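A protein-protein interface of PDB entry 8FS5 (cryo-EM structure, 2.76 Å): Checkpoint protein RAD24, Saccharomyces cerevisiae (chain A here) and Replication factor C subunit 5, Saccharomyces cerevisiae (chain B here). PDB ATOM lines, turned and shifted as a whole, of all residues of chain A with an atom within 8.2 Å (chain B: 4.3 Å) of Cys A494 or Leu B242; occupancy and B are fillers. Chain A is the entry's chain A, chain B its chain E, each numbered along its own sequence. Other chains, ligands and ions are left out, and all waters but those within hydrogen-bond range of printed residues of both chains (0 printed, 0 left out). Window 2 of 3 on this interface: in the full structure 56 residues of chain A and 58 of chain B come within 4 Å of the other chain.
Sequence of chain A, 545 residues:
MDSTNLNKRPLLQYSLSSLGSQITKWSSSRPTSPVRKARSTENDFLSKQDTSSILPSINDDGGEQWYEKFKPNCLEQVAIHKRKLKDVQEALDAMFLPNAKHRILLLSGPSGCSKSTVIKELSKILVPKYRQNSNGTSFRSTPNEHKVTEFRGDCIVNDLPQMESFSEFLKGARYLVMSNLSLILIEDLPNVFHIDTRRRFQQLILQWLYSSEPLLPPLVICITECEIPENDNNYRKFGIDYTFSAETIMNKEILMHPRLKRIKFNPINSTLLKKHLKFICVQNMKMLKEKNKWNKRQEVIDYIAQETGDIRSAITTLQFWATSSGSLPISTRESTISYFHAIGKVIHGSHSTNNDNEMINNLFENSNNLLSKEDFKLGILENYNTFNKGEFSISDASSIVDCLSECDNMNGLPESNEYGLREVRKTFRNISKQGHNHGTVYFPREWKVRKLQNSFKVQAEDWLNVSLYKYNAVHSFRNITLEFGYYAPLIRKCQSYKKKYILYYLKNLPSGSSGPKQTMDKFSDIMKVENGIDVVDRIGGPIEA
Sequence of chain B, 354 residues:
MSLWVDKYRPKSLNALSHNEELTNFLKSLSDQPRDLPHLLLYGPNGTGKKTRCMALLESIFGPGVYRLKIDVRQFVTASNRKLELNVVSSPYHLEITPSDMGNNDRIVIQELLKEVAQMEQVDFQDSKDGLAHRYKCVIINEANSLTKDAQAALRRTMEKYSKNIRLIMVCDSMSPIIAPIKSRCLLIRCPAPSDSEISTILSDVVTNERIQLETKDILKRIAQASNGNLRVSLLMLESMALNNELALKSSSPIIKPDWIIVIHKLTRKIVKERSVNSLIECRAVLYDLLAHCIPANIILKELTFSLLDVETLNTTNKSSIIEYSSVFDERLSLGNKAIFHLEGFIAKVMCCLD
Of the 14 printed residues of chain A, 5 touch a printed residue of chain B. Printed residues of chain A that touch a printed residue of chain B: Tyr A487, Leu A490, Ile A491, Cys A494 and Gln A495. Hydrophobic or aromatic side chains of chain A within 4 Å of the printed part of chain B: Tyr A487 and Ile A491. Printed residues of chain B that touch a printed residue of chain A: Glu B238, Ser B239, Leu B242 and Asn B243. Along chain B the printed residues that touch a printed residue of chain A span positions 238 to 243. Among the printed residues, no Asp or Glu carboxylate lies within 4 Å of a Lys or Arg side-chain nitrogen of the other chain.
O of Ser B239 sits at hydrogen-bond distance from ND2 of Asn B243, at 2.7 Å. NH1 of Arg A492 lies close to NE2 of Gln A495 (3.3 Å).
The side-chain sulfur (SG) of Cys A494 lies within hydrogen-bond range of the side-chain amide nitrogen (ND2) of Asn B243, at 3.8 Å. O of Leu B242 sits at hydrogen-bond distance from SG of Cys A494, 3.2 Å away.
Among the printed residues, merely in contact across the chains: Tyr A487 with Ser B239 (3.3 Å), Leu A490 with Asn B243 (3.9 Å), Ile A491 with Glu B238 (3.4 Å), Ile A491 with Ser B239 (3.6 Å), Ile A491 with Leu B242 (3.6 Å), Gln A495 with Glu B238 (3.7 Å) and Gln A495 with Leu B242 (3.5 Å).
Of the printed residues of chain B, Leu A490 touches Asn B243. Printed residues of chain B within 4 Å of Ile A491: Glu B238, Ser B239 and Leu B242. Of chain B, only Leu B242 (3.2 Å) and Asn B243 (3.8 Å) come within 4 Å of Cys A494. Of the printed residues of chain B, Gln A495 touches Glu B238 and Leu B242. Of the printed residues of chain A, Glu B238 touches Ile A491 (3.4 Å) and Gln A495 (3.7 Å). No residue of chain A comes within 4 Å of Ala B241. Leu B242 touches three residues of chain A. The nearest residue of chain A that does not touch Leu B242 is Leu A490 (5.1 Å).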
ATOM      1  N   TYR A 487      -4.571  -0.153 -15.087  1.00  0.00           N
ATOM      2  CA  TYR A 487      -4.084  -1.346 -15.765  1.00  0.00           C
ATOM      3  C   TYR A 487      -4.830  -2.610 -15.365  1.00  0.00           C
ATOM      4  O   TYR A 487      -5.183  -3.408 -16.240  1.00  0.00           O
ATOM      5  CB  TYR A 487      -2.591  -1.542 -15.482  1.00  0.00           C
ATOM      6  CG  TYR A 487      -1.683  -0.644 -16.288  1.00  0.00           C
ATOM      7  CD1 TYR A 487      -1.741  -0.630 -17.674  1.00  0.00           C
ATOM      8  CD2 TYR A 487      -0.768   0.191 -15.661  1.00  0.00           C
ATOM      9  CE1 TYR A 487      -0.911   0.188 -18.414  1.00  0.00           C
ATOM     10  CE2 TYR A 487       0.066   1.015 -16.394  1.00  0.00           C
ATOM     11  CZ  TYR A 487      -0.011   1.010 -17.770  1.00  0.00           C
ATOM     12  OH  TYR A 487       0.816   1.827 -18.505  1.00  0.00           O
ATOM     13  N   ALA A 488      -5.075  -2.808 -14.071  1.00  0.00           N
ATOM     14  CA  ALA A 488      -5.750  -3.999 -13.567  1.00  0.00           C
ATOM     15  C   ALA A 488      -7.181  -4.134 -14.091  1.00  0.00           C
ATOM     16  O   ALA A 488      -7.570  -5.242 -14.485  1.00  0.00           O
ATOM     17  CB  ALA A 488      -5.730  -4.017 -12.036  1.00  0.00           C
ATOM     18  N   PRO A 489      -8.023  -3.064 -14.093  1.00  0.00           N
ATOM     19  CA  PRO A 489      -9.320  -3.190 -14.772  1.00  0.00           C
ATOM     20  C   PRO A 489      -9.161  -3.422 -16.265  1.00  0.00           C
ATOM     21  O   PRO A 489      -9.912  -4.201 -16.855  1.00  0.00           O
ATOM     22  CB  PRO A 489     -10.012  -1.853 -14.478  1.00  0.00           C
ATOM     23  CG  PRO A 489      -8.914  -0.922 -14.181  1.00  0.00           C
ATOM     24  CD  PRO A 489      -7.905  -1.742 -13.448  1.00  0.00           C
ATOM     25  N   LEU A 490      -8.164  -2.776 -16.879  1.00  0.00           N
ATOM     26  CA  LEU A 490      -7.912  -2.952 -18.304  1.00  0.00           C
ATOM     27  C   LEU A 490      -7.484  -4.371 -18.652  1.00  0.00           C
ATOM     28  O   LEU A 490      -7.524  -4.739 -19.830  1.00  0.00           O
ATOM     29  CB  LEU A 490      -6.843  -1.967 -18.782  1.00  0.00           C
ATOM     30  CG  LEU A 490      -6.975  -1.436 -20.210  1.00  0.00           C
ATOM     31  CD1 LEU A 490      -8.148  -0.475 -20.323  1.00  0.00           C
ATOM     32  CD2 LEU A 490      -5.684  -0.765 -20.653  1.00  0.00           C
ATOM     33  N   ILE A 491      -7.077  -5.165 -17.663  1.00  0.00           N
ATOM     34  CA  ILE A 491      -6.731  -6.567 -17.855  1.00  0.00           C
ATOM     35  C   ILE A 491      -7.903  -7.476 -17.508  1.00  0.00           C
ATOM     36  O   ILE A 491      -8.227  -8.403 -18.257  1.00  0.00           O
ATOM     37  CB  ILE A 491      -5.478  -6.952 -17.035  1.00  0.00           C
ATOM     38  CG1 ILE A 491      -4.250  -6.218 -17.575  1.00  0.00           C
ATOM     39  CG2 ILE A 491      -5.257  -8.457 -17.051  1.00  0.00           C
ATOM     40  CD1 ILE A 491      -3.998  -6.455 -19.043  1.00  0.00           C
ATOM     41  N   ARG A 492      -8.561  -7.215 -16.377  1.00  0.00           N
ATOM     42  CA  ARG A 492      -9.657  -8.074 -15.939  1.00  0.00           C
ATOM     43  C   ARG A 492     -10.867  -7.958 -16.861  1.00  0.00           C
ATOM     44  O   ARG A 492     -11.489  -8.970 -17.206  1.00  0.00           O
ATOM     45  CB  ARG A 492     -10.037  -7.744 -14.497  1.00  0.00           C
ATOM     46  CG  ARG A 492      -9.079  -8.332 -13.472  1.00  0.00           C
ATOM     47  CD  ARG A 492      -9.013  -9.846 -13.600  1.00  0.00           C
ATOM     48  NE  ARG A 492      -8.055 -10.443 -12.677  1.00  0.00           N
ATOM     49  CZ  ARG A 492      -6.789 -10.700 -12.975  1.00  0.00           C
ATOM     50  NH1 ARG A 492      -6.289 -10.420 -14.167  1.00  0.00           N
ATOM     51  NH2 ARG A 492      -6.005 -11.254 -12.055  1.00  0.00           N
ATOM     52  N   LYS A 493     -11.223  -6.736 -17.269  1.00  0.00           N
ATOM     53  CA  LYS A 493     -12.356  -6.557 -18.170  1.00  0.00           C
ATOM     54  C   LYS A 493     -12.034  -7.077 -19.567  1.00  0.00           C
ATOM     55  O   LYS A 493     -12.938  -7.432 -20.331  1.00  0.00           O
ATOM     56  CB  LYS A 493     -12.763  -5.081 -18.213  1.00  0.00           C
ATOM     57  CG  LYS A 493     -12.102  -4.270 -19.317  1.00  0.00           C
ATOM     58  CD  LYS A 493     -12.783  -2.927 -19.512  1.00  0.00           C
ATOM     59  CE  LYS A 493     -11.821  -1.907 -20.099  1.00  0.00           C
ATOM     60  NZ  LYS A 493     -11.941  -0.578 -19.439  1.00  0.00           N
ATOM     61  N   CYS A 494     -10.743  -7.067 -19.909  1.00  0.00           N
ATOM     62  CA  CYS A 494     -10.307  -7.546 -21.245  1.00  0.00           C
ATOM     63  C   CYS A 494     -10.237  -9.071 -21.198  1.00  0.00           C
ATOM     64  O   CYS A 494     -10.391  -9.696 -22.261  1.00  0.00           O
ATOM     65  CB  CYS A 494      -8.948  -6.961 -21.609  1.00  0.00           C
ATOM     66  SG  CYS A 494      -8.664  -6.843 -23.394  1.00  0.00           S
ATOM     67  N   GLN A 495     -10.004  -9.639 -20.014  1.00  0.00           N
ATOM     68  CA  GLN A 495     -10.025 -11.118 -19.864  1.00  0.00           C
ATOM     69  C   GLN A 495     -11.483 -11.578 -19.786  1.00  0.00           C
ATOM     70  O   GLN A 495     -11.757 -12.738 -20.133  1.00  0.00           O
ATOM     71  CB  GLN A 495      -9.277 -11.554 -18.605  1.00  0.00           C
ATOM     72  CG  GLN A 495      -7.764 -11.544 -18.753  1.00  0.00           C
ATOM     73  CD  GLN A 495      -7.074 -11.916 -17.464  1.00  0.00           C
ATOM     74  OE1 GLN A 495      -5.849 -11.966 -17.386  1.00  0.00           O
ATOM     75  NE2 GLN A 495      -7.863 -12.182 -16.436  1.00  0.00           N
ATOM     76  N   SER A 496     -12.369 -10.691 -19.327  1.00  0.00           N
ATOM     77  CA  SER A 496     -13.809 -11.018 -19.177  1.00  0.00           C
ATOM     78  C   SER A 496     -14.539 -10.802 -20.508  1.00  0.00           C
ATOM     79  O   SER A 496     -15.621 -11.391 -20.685  1.00  0.00           O
ATOM     80  CB  SER A 496     -14.432 -10.214 -18.065  1.00  0.00           C
ATOM     81  OG  SER A 496     -13.801 -10.496 -16.826  1.00  0.00           O
ATOM     82  N   TYR A 497     -13.963 -10.001 -21.407  1.00  0.00           N
ATOM     83  CA  TYR A 497     -14.585  -9.760 -22.736  1.00  0.00           C
ATOM     84  C   TYR A 497     -14.221 -10.902 -23.688  1.00  0.00           C
ATOM     85  O   TYR A 497     -13.845 -10.613 -24.840  1.00  0.00           O
ATOM     86  CB  TYR A 497     -14.137  -8.420 -23.326  1.00  0.00           C
ATOM     87  CG  TYR A 497     -14.717  -7.199 -22.658  1.00  0.00           C
ATOM     88  CD1 TYR A 497     -15.661  -7.309 -21.652  1.00  0.00           C
ATOM     89  CD2 TYR A 497     -14.303  -5.928 -23.019  1.00  0.00           C
ATOM     90  CE1 TYR A 497     -16.187  -6.190 -21.028  1.00  0.00           C
ATOM     91  CE2 TYR A 497     -14.819  -4.798 -22.408  1.00  0.00           C
ATOM     92  CZ  TYR A 497     -15.764  -4.929 -21.409  1.00  0.00           C
ATOM     93  OH  TYR A 497     -16.281  -3.812 -20.798  1.00  0.00           O
ATOM     94  N   LYS A 498     -14.337 -12.151 -23.224  1.00  0.00           N
ATOM     95  CA  LYS A 498     -14.035 -13.304 -24.074  1.00  0.00           C
ATOM     96  C   LYS A 498     -14.499 -14.593 -23.401  1.00  0.00           C
ATOM     97  O   LYS A 498     -13.692 -15.371 -22.891  1.00  0.00           O
ATOM     98  CB  LYS A 498     -12.535 -13.392 -24.403  1.00  0.00           C
ATOM     99  CG  LYS A 498     -11.592 -12.993 -23.275  1.00  0.00           C
ATOM    100  CD  LYS A 498     -10.137 -13.038 -23.722  1.00  0.00           C
ATOM    101  CE  LYS A 498      -9.783 -14.370 -24.368  1.00  0.00           C
ATOM    102  NZ  LYS A 498     -10.126 -15.526 -23.496  1.00  0.00           N
ATOM    103  N   VAL A 535     -13.144  -7.799  -9.816  1.00  0.00           N
ATOM    104  CA  VAL A 535     -13.562  -6.450 -10.178  1.00  0.00           C
ATOM    105  C   VAL A 535     -13.054  -6.134 -11.579  1.00  0.00           C
ATOM    106  O   VAL A 535     -12.000  -6.626 -11.999  1.00  0.00           O
ATOM    107  CB  VAL A 535     -13.056  -5.427  -9.149  1.00  0.00           C
ATOM    108  CG1 VAL A 535     -13.630  -5.734  -7.775  1.00  0.00           C
ATOM    109  CG2 VAL A 535     -11.540  -5.429  -9.095  1.00  0.00           C
ATOM    110  N   VAL A 536     -13.814  -5.326 -12.314  1.00  0.00           N
ATOM    111  CA  VAL A 536     -13.475  -4.982 -13.690  1.00  0.00           C
ATOM    112  C   VAL A 536     -13.522  -3.487 -13.958  1.00  0.00           C
ATOM    113  O   VAL A 536     -13.170  -3.064 -15.071  1.00  0.00           O
ATOM    114  CB  VAL A 536     -14.384  -5.723 -14.695  1.00  0.00           C
ATOM    115  CG1 VAL A 536     -13.943  -7.171 -14.843  1.00  0.00           C
ATOM    116  CG2 VAL A 536     -15.837  -5.644 -14.253  1.00  0.00           C
ATOM    117  N   GLU B 238       1.070  -6.916 -20.951  1.00  0.00           N
ATOM    118  CA  GLU B 238      -0.212  -7.603 -20.859  1.00  0.00           C
ATOM    119  C   GLU B 238      -1.353  -6.765 -21.421  1.00  0.00           C
ATOM    120  O   GLU B 238      -2.262  -7.319 -22.052  1.00  0.00           O
ATOM    121  CB  GLU B 238      -0.497  -7.978 -19.404  1.00  0.00           C
ATOM    122  CG  GLU B 238      -1.539  -9.067 -19.227  1.00  0.00           C
ATOM    123  CD  GLU B 238      -1.644  -9.545 -17.792  1.00  0.00           C
ATOM    124  OE1 GLU B 238      -0.872  -9.053 -16.942  1.00  0.00           O
ATOM    125  OE2 GLU B 238      -2.496 -10.414 -17.513  1.00  0.00           O
ATOM    126  N   SER B 239      -1.323  -5.445 -21.217  1.00  0.00           N
ATOM    127  CA  SER B 239      -2.352  -4.570 -21.766  1.00  0.00           C
ATOM    128  C   SER B 239      -2.383  -4.588 -23.291  1.00  0.00           C
ATOM    129  O   SER B 239      -3.439  -4.835 -23.883  1.00  0.00           O
ATOM    130  CB  SER B 239      -2.143  -3.137 -21.268  1.00  0.00           C
ATOM    131  OG  SER B 239      -1.793  -3.119 -19.895  1.00  0.00           O
ATOM    132  N   MET B 240      -1.242  -4.361 -23.944  1.00  0.00           N
ATOM    133  CA  MET B 240      -1.195  -4.371 -25.402  1.00  0.00           C
ATOM    134  C   MET B 240      -1.297  -5.785 -25.958  1.00  0.00           C
ATOM    135  O   MET B 240      -1.533  -5.963 -27.158  1.00  0.00           O
ATOM    136  CB  MET B 240       0.075  -3.686 -25.918  1.00  0.00           C
ATOM    137  CG  MET B 240       0.473  -2.434 -25.156  1.00  0.00           C
ATOM    138  SD  MET B 240       2.095  -1.791 -25.616  1.00  0.00           S
ATOM    139  CE  MET B 240       2.327  -2.534 -27.230  1.00  0.00           C
ATOM    140  N   ALA B 241      -1.129  -6.799 -25.110  1.00  0.00           N
ATOM    141  CA  ALA B 241      -1.357  -8.179 -25.512  1.00  0.00           C
ATOM    142  C   ALA B 241      -2.842  -8.509 -25.574  1.00  0.00           C
ATOM    143  O   ALA B 241      -3.331  -8.979 -26.605  1.00  0.00           O
ATOM    144  CB  ALA B 241      -0.636  -9.136 -24.553  1.00  0.00           C
ATOM    145  N   LEU B 242      -3.582  -8.266 -24.489  1.00  0.00           N
ATOM    146  CA  LEU B 242      -5.008  -8.571 -24.496  1.00  0.00           C
ATOM    147  C   LEU B 242      -5.815  -7.583 -25.330  1.00  0.00           C
ATOM    148  O   LEU B 242      -6.869  -7.954 -25.857  1.00  0.00           O
ATOM    149  CB  LEU B 242      -5.573  -8.638 -23.067  1.00  0.00           C
ATOM    150  CG  LEU B 242      -5.236  -9.768 -22.073  1.00  0.00           C
ATOM    151  CD1 LEU B 242      -3.763 -10.166 -21.984  1.00  0.00           C
ATOM    152  CD2 LEU B 242      -5.780  -9.427 -20.687  1.00  0.00           C
ATOM    153  N   ASN B 243      -5.344  -6.344 -25.485  1.00  0.00           N
ATOM    154  CA  ASN B 243      -6.048  -5.350 -26.284  1.00  0.00           C
ATOM    155  C   ASN B 243      -5.730  -5.462 -27.772  1.00  0.00           C
ATOM    156  O   ASN B 243      -6.253  -4.677 -28.571  1.00  0.00           O
ATOM    157  CB  ASN B 243      -5.736  -3.941 -25.775  1.00  0.00           C
ATOM    158  CG  ASN B 243      -6.451  -3.619 -24.475  1.00  0.00           C
ATOM    159  OD1 ASN B 243      -7.422  -2.866 -24.453  1.00  0.00           O
ATOM    160  ND2 ASN B 243      -5.969  -4.197 -23.380  1.00  0.00           N
ATOM    161  N   ASN B 244      -4.893  -6.423 -28.161  1.00  0.00           N
ATOM    162  CA  ASN B 244      -4.603  -6.646 -29.571  1.00  0.00           C
ATOM    163  C   ASN B 244      -4.765  -8.118 -29.928  1.00  0.00           C
ATOM    164  O   ASN B 244      -4.128  -8.605 -30.868  1.00  0.00           O
ATOM    165  CB  ASN B 244      -3.191  -6.167 -29.915  1.00  0.00           C
ATOM    166  CG  ASN B 244      -3.127  -4.672 -30.154  1.00  0.00           C
ATOM    167  OD1 ASN B 244      -2.046  -4.093 -30.249  1.00  0.00           O
ATOM    168  ND2 ASN B 244      -4.289  -4.037 -30.243  1.00  0.00           N
ATOM    169  N   GLU B 245      -5.623  -8.821 -29.182  1.00  0.00           N
ATOM    170  CA  GLU B 245      -5.921 -10.234 -29.402  1.00  0.00           C
ATOM    171  C   GLU B 245      -4.663 -11.096 -29.416  1.00  0.00           C
ATOM    172  O   GLU B 245      -4.522 -11.974 -30.275  1.00  0.00           O
ATOM    173  CB  GLU B 245      -6.701 -10.424 -30.707  1.00  0.00           C
ATOM    174  CG  GLU B 245      -7.825  -9.421 -30.926  1.00  0.00           C
ATOM    175  CD  GLU B 245      -9.001  -9.645 -29.994  1.00  0.00           C
ATOM    176  OE1 GLU B 245      -9.170 -10.783 -29.505  1.00  0.00           O
ATOM    177  OE2 GLU B 245      -9.759  -8.683 -29.752  1.00  0.00           O
